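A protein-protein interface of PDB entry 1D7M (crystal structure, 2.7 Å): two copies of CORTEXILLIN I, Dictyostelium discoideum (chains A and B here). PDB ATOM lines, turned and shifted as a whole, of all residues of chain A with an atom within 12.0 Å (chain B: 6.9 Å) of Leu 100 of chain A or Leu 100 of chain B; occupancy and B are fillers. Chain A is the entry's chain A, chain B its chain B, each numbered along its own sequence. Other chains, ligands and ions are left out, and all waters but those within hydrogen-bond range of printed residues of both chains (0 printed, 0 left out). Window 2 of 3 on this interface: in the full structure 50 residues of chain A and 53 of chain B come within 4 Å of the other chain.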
ATOM      1  N   ALA A  91      13.431  28.660   2.177  1.00  0.00           N
ATOM      2  CA  ALA A  91      14.524  27.998   1.465  1.00  0.00           C
ATOM      3  C   ALA A  91      14.744  26.589   2.009  1.00  0.00           C
ATOM      4  O   ALA A  91      14.691  25.604   1.271  1.00  0.00           O
ATOM      5  CB  ALA A  91      15.787  28.809   1.610  1.00  0.00           C
ATOM      6  N   GLU A  92      14.988  26.499   3.311  1.00  0.00           N
ATOM      7  CA  GLU A  92      15.210  25.215   3.958  1.00  0.00           C
ATOM      8  C   GLU A  92      14.160  24.184   3.537  1.00  0.00           C
ATOM      9  O   GLU A  92      14.481  23.033   3.246  1.00  0.00           O
ATOM     10  CB  GLU A  92      15.173  25.398   5.479  1.00  0.00           C
ATOM     11  CG  GLU A  92      15.326  24.096   6.251  1.00  0.00           C
ATOM     12  CD  GLU A  92      15.296  24.253   7.772  1.00  0.00           C
ATOM     13  OE1 GLU A  92      14.229  24.566   8.347  1.00  0.00           O
ATOM     14  OE2 GLU A  92      16.357  24.047   8.399  1.00  0.00           O
ATOM     15  N   ALA A  93      12.906  24.609   3.494  1.00  0.00           N
ATOM     16  CA  ALA A  93      11.821  23.715   3.132  1.00  0.00           C
ATOM     17  C   ALA A  93      11.760  23.373   1.652  1.00  0.00           C
ATOM     18  O   ALA A  93      11.502  22.218   1.297  1.00  0.00           O
ATOM     19  CB  ALA A  93      10.517  24.317   3.564  1.00  0.00           C
ATOM     20  N   ILE A  94      11.975  24.350   0.777  1.00  0.00           N
ATOM     21  CA  ILE A  94      11.907  23.994  -0.631  1.00  0.00           C
ATOM     22  C   ILE A  94      13.066  23.077  -0.927  1.00  0.00           C
ATOM     23  O   ILE A  94      13.024  22.302  -1.878  1.00  0.00           O
ATOM     24  CB  ILE A  94      11.900  25.225  -1.591  1.00  0.00           C
ATOM     25  CG1 ILE A  94      13.130  26.112  -1.391  1.00  0.00           C
ATOM     26  CG2 ILE A  94      10.624  26.002  -1.384  1.00  0.00           C
ATOM     27  CD1 ILE A  94      13.257  27.230  -2.436  1.00  0.00           C
ATOM     28  N   ASP A  95      14.090  23.123  -0.086  1.00  0.00           N
ATOM     29  CA  ASP A  95      15.183  22.224  -0.343  1.00  0.00           C
ATOM     30  C   ASP A  95      14.909  20.847   0.193  1.00  0.00           C
ATOM     31  O   ASP A  95      15.301  19.857  -0.418  1.00  0.00           O
ATOM     32  CB  ASP A  95      16.500  22.748   0.180  1.00  0.00           C
ATOM     33  CG  ASP A  95      17.525  22.773  -0.902  1.00  0.00           C
ATOM     34  OD1 ASP A  95      18.710  22.526  -0.616  1.00  0.00           O
ATOM     35  OD2 ASP A  95      17.106  23.037  -2.052  1.00  0.00           O
ATOM     36  N   GLU A  96      14.230  20.762   1.328  1.00  0.00           N
ATOM     37  CA  GLU A  96      13.908  19.449   1.848  1.00  0.00           C
ATOM     38  C   GLU A  96      12.954  18.757   0.899  1.00  0.00           C
ATOM     39  O   GLU A  96      12.952  17.531   0.796  1.00  0.00           O
ATOM     40  CB  GLU A  96      13.299  19.551   3.226  1.00  0.00           C
ATOM     41  CG  GLU A  96      14.357  19.434   4.257  1.00  0.00           C
ATOM     42  CD  GLU A  96      14.161  20.421   5.339  1.00  0.00           C
ATOM     43  OE1 GLU A  96      13.065  20.395   5.935  1.00  0.00           O
ATOM     44  OE2 GLU A  96      15.091  21.216   5.586  1.00  0.00           O
ATOM     45  N   LYS A  97      12.141  19.546   0.206  1.00  0.00           N
ATOM     46  CA  LYS A  97      11.224  18.988  -0.771  1.00  0.00           C
ATOM     47  C   LYS A  97      12.148  18.441  -1.870  1.00  0.00           C
ATOM     48  O   LYS A  97      12.133  17.248  -2.158  1.00  0.00           O
ATOM     49  CB  LYS A  97      10.305  20.083  -1.328  1.00  0.00           C
ATOM     50  CG  LYS A  97       9.078  19.567  -2.067  1.00  0.00           C
ATOM     51  CD  LYS A  97       8.699  20.476  -3.239  1.00  0.00           C
ATOM     52  CE  LYS A  97       7.455  19.955  -3.960  1.00  0.00           C
ATOM     53  NZ  LYS A  97       7.046  20.785  -5.135  1.00  0.00           N
ATOM     54  N   SER A  98      12.979  19.305  -2.458  1.00  0.00           N
ATOM     55  CA  SER A  98      13.907  18.870  -3.511  1.00  0.00           C
ATOM     56  C   SER A  98      14.588  17.535  -3.189  1.00  0.00           C
ATOM     57  O   SER A  98      14.344  16.531  -3.864  1.00  0.00           O
ATOM     58  CB  SER A  98      14.982  19.931  -3.773  1.00  0.00           C
ATOM     59  OG  SER A  98      14.426  21.101  -4.342  1.00  0.00           O
ATOM     60  N   LYS A  99      15.452  17.523  -2.176  1.00  0.00           N
ATOM     61  CA  LYS A  99      16.136  16.293  -1.781  1.00  0.00           C
ATOM     62  C   LYS A  99      15.163  15.134  -1.631  1.00  0.00           C
ATOM     63  O   LYS A  99      15.395  14.066  -2.191  1.00  0.00           O
ATOM     64  CB  LYS A  99      16.910  16.481  -0.469  1.00  0.00           C
ATOM     65  CG  LYS A  99      18.045  17.481  -0.580  1.00  0.00           C
ATOM     66  CD  LYS A  99      19.240  17.146   0.310  1.00  0.00           C
ATOM     67  CE  LYS A  99      20.423  18.043  -0.057  1.00  0.00           C
ATOM     68  NZ  LYS A  99      21.699  17.625   0.583  1.00  0.00           N
ATOM     69  N   LEU A 100      14.074  15.331  -0.884  1.00  0.00           N
ATOM     70  CA  LEU A 100      13.114  14.246  -0.715  1.00  0.00           C
ATOM     71  C   LEU A 100      12.931  13.604  -2.085  1.00  0.00           C
ATOM     72  O   LEU A 100      13.161  12.412  -2.238  1.00  0.00           O
ATOM     73  CB  LEU A 100      11.764  14.742  -0.183  1.00  0.00           C
ATOM     74  CG  LEU A 100      11.099  13.741   0.772  1.00  0.00           C
ATOM     75  CD1 LEU A 100      11.825  13.798   2.116  1.00  0.00           C
ATOM     76  CD2 LEU A 100       9.615  14.056   0.942  1.00  0.00           C
ATOM     77  N   GLU A 101      12.556  14.383  -3.096  1.00  0.00           N
ATOM     78  CA  GLU A 101      12.392  13.802  -4.426  1.00  0.00           C
ATOM     79  C   GLU A 101      13.712  13.357  -5.099  1.00  0.00           C
ATOM     80  O   GLU A 101      13.694  12.277  -5.731  1.00  0.00           O
ATOM     81  CB  GLU A 101      11.593  14.751  -5.342  1.00  0.00           C
ATOM     82  CG  GLU A 101      11.571  16.202  -4.887  1.00  0.00           C
ATOM     83  CD  GLU A 101      10.383  16.986  -5.431  1.00  0.00           C
ATOM     84  OE1 GLU A 101       9.232  16.557  -5.201  1.00  0.00           O
ATOM     85  OE2 GLU A 101      10.602  18.032  -6.079  1.00  0.00           O
ATOM     86  OXT GLU A 101      14.744  14.057  -4.999  1.00  0.00           O
ATOM     87  N   ASP B  95       3.783  21.095   3.203  1.00  0.00           N
ATOM     88  CA  ASP B  95       2.780  20.110   2.862  1.00  0.00           C
ATOM     89  C   ASP B  95       3.140  19.290   1.652  1.00  0.00           C
ATOM     90  O   ASP B  95       2.929  18.084   1.649  1.00  0.00           O
ATOM     91  CB  ASP B  95       1.418  20.716   2.599  1.00  0.00           C
ATOM     92  CG  ASP B  95       0.400  19.651   2.225  1.00  0.00           C
ATOM     93  OD1 ASP B  95      -0.505  19.936   1.419  1.00  0.00           O
ATOM     94  OD2 ASP B  95       0.518  18.518   2.746  1.00  0.00           O
ATOM     95  N   GLU B  96       3.650  19.924   0.605  1.00  0.00           N
ATOM     96  CA  GLU B  96       4.022  19.146  -0.560  1.00  0.00           C
ATOM     97  C   GLU B  96       4.985  18.071  -0.076  1.00  0.00           C
ATOM     98  O   GLU B  96       4.960  16.947  -0.565  1.00  0.00           O
ATOM     99  CB  GLU B  96       4.636  20.060  -1.609  1.00  0.00           C
ATOM    100  CG  GLU B  96       3.586  20.993  -2.183  1.00  0.00           C
ATOM    101  CD  GLU B  96       4.172  22.256  -2.765  1.00  0.00           C
ATOM    102  OE1 GLU B  96       5.188  22.155  -3.483  1.00  0.00           O
ATOM    103  OE2 GLU B  96       3.610  23.345  -2.513  1.00  0.00           O
ATOM    104  N   LYS B  97       5.800  18.422   0.918  1.00  0.00           N
ATOM    105  CA  LYS B  97       6.754  17.496   1.539  1.00  0.00           C
ATOM    106  C   LYS B  97       5.983  16.372   2.254  1.00  0.00           C
ATOM    107  O   LYS B  97       6.193  15.176   2.020  1.00  0.00           O
ATOM    108  CB  LYS B  97       7.600  18.245   2.572  1.00  0.00           C
ATOM    109  CG  LYS B  97       9.086  18.221   2.303  1.00  0.00           C
ATOM    110  CD  LYS B  97       9.859  18.040   3.598  1.00  0.00           C
ATOM    111  CE  LYS B  97       9.368  16.802   4.338  1.00  0.00           C
ATOM    112  NZ  LYS B  97      10.311  16.346   5.389  1.00  0.00           N
ATOM    113  N   SER B  98       5.097  16.796   3.145  1.00  0.00           N
ATOM    114  CA  SER B  98       4.241  15.906   3.916  1.00  0.00           C
ATOM    115  C   SER B  98       3.612  14.832   3.022  1.00  0.00           C
ATOM    116  O   SER B  98       3.710  13.636   3.309  1.00  0.00           O
ATOM    117  CB  SER B  98       3.154  16.743   4.591  1.00  0.00           C
ATOM    118  OG  SER B  98       2.146  15.930   5.154  1.00  0.00           O
ATOM    119  N   LYS B  99       2.975  15.280   1.939  1.00  0.00           N
ATOM    120  CA  LYS B  99       2.319  14.401   0.970  1.00  0.00           C
ATOM    121  C   LYS B  99       3.326  13.520   0.232  1.00  0.00           C
ATOM    122  O   LYS B  99       3.000  12.402  -0.163  1.00  0.00           O
ATOM    123  CB  LYS B  99       1.497  15.244  -0.018  1.00  0.00           C
ATOM    124  CG  LYS B  99       0.364  16.023   0.665  1.00  0.00           C
ATOM    125  CD  LYS B  99      -0.638  16.633  -0.318  1.00  0.00           C
ATOM    126  CE  LYS B  99       0.007  17.637  -1.277  1.00  0.00           C
ATOM    127  NZ  LYS B  99       0.617  18.831  -0.614  1.00  0.00           N
ATOM    128  N   LEU B 100       4.547  14.016   0.040  1.00  0.00           N
ATOM    129  CA  LEU B 100       5.570  13.206  -0.615  1.00  0.00           C
ATOM    130  C   LEU B 100       5.984  12.041   0.290  1.00  0.00           C
ATOM    131  O   LEU B 100       6.599  11.082  -0.169  1.00  0.00           O
ATOM    132  CB  LEU B 100       6.803  14.037  -0.995  1.00  0.00           C
ATOM    133  CG  LEU B 100       6.676  14.931  -2.239  1.00  0.00           C
ATOM    134  CD1 LEU B 100       7.860  14.689  -3.178  1.00  0.00           C
ATOM    135  CD2 LEU B 100       5.359  14.640  -2.955  1.00  0.00           C
ATOM    136  N   GLU B 101       5.653  12.127   1.580  1.00  0.00           N
ATOM    137  CA  GLU B 101       5.960  11.045   2.522  1.00  0.00           C
ATOM    138  C   GLU B 101       5.299   9.749   2.044  1.00  0.00           C
ATOM    139  O   GLU B 101       6.022   8.753   1.816  1.00  0.00           O
ATOM    140  CB  GLU B 101       5.431  11.369   3.926  1.00  0.00           C
ATOM    141  CG  GLU B 101       6.491  11.493   5.014  1.00  0.00           C
ATOM    142  CD  GLU B 101       7.522  12.569   4.711  1.00  0.00           C
ATOM    143  OE1 GLU B 101       7.980  13.238   5.664  1.00  0.00           O
ATOM    144  OE2 GLU B 101       7.883  12.741   3.527  1.00  0.00           O
ATOM    145  OXT GLU B 101       4.054   9.751   1.918  1.00  0.00           O
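NZ of Lys 97 of chain A is in salt-bridge range of OE1 of Glu 96 of chain B (2.8 Å).
The side-chain amino group (NZ) of Lys 97 of chain B lies within salt-bridge range of the side-chain carboxylate (OE1) of Glu 101 of chain B, 3.9 Å away.
CD of Lys 97 of chain B touches CB of Glu 96 of chain A, 3.8 Å away.
Lys 97 of chain A touches Lys 97 of chain B (CA to CG, 3.8 Å).
Lys 97 of chain B touches Leu 100 of chain A.
Leu 100 of chain A touches Leu 100 of chain B (CD2 to CB, 3.4 Å).
CD2 of Leu 100 of chain A touches OE2 of Glu 101 of chain B (3.4 Å).
Glu 101 of chain A touches Leu 100 of chain B.
Glu 92 of chain A touches none of the printed residues of chain B.
Of the printed residues of chain B, Glu 96 of chain A touches Lys 97.
Leu 100 of chain A touches just these residues of chain B: Lys 97, Leu 100 and Glu 101.
Of the printed residues of chain B, Glu 101 of chain A touches Leu 100 (3.1 Å).
Lys 97 of chain B touches just these residues of chain A: Glu 96 (3.8 Å), Lys 97 (3.8 Å) and Leu 100 (3.8 Å).
No residue of chain A comes within 4 Å of Lys 99 of chain B.
Of chain A, only Leu 100 and Glu 101 come within 4 Å of Leu 100 of chain B.
Printed residues of chain A within 4 Å of Glu 101 of chain B: Leu 100.
The nearest residue of chain B that does not touch Leu 100 of chain A is Glu 96 of chain B (5.7 Å).
The nearest residue of chain A that does not touch Leu 100 of chain B is Lys 97 of chain A (5.1 Å).
The nearest printed residue of chain B that does not touch Glu 101 of chain A is Glu 96 of chain B (6.3 Å).
Of the 11 printed residues of chain A, 4 touch a printed residue of chain B.
Of the 7 printed residues of chain B, 4 touch a printed residue of chain A.
Glu 96 of chain A touches Lys 97 of chain B, and with the chains exchanged Lys 97 of chain A touches Glu 96 of chain B.
Lys 97 of chain A touches its own counterpart, Lys 97 of chain B.
Leu 100 of chain A touches Lys 97 of chain B, but with the chains exchanged Lys 97 of chain A does not touch Leu 100 of chain B (5.1 Å).
Leu 100 of chain A touches Glu 101 of chain B, and with the chains exchanged Glu 101 of chain A touches Leu 100 of chain B.
Positions printed for both chains: 95, 96, 97, 98, 99, 100 and 101.
Of the 7 pairs that touch across the chains among the printed residues, 6 have their exchanged pair printed and touching as well.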
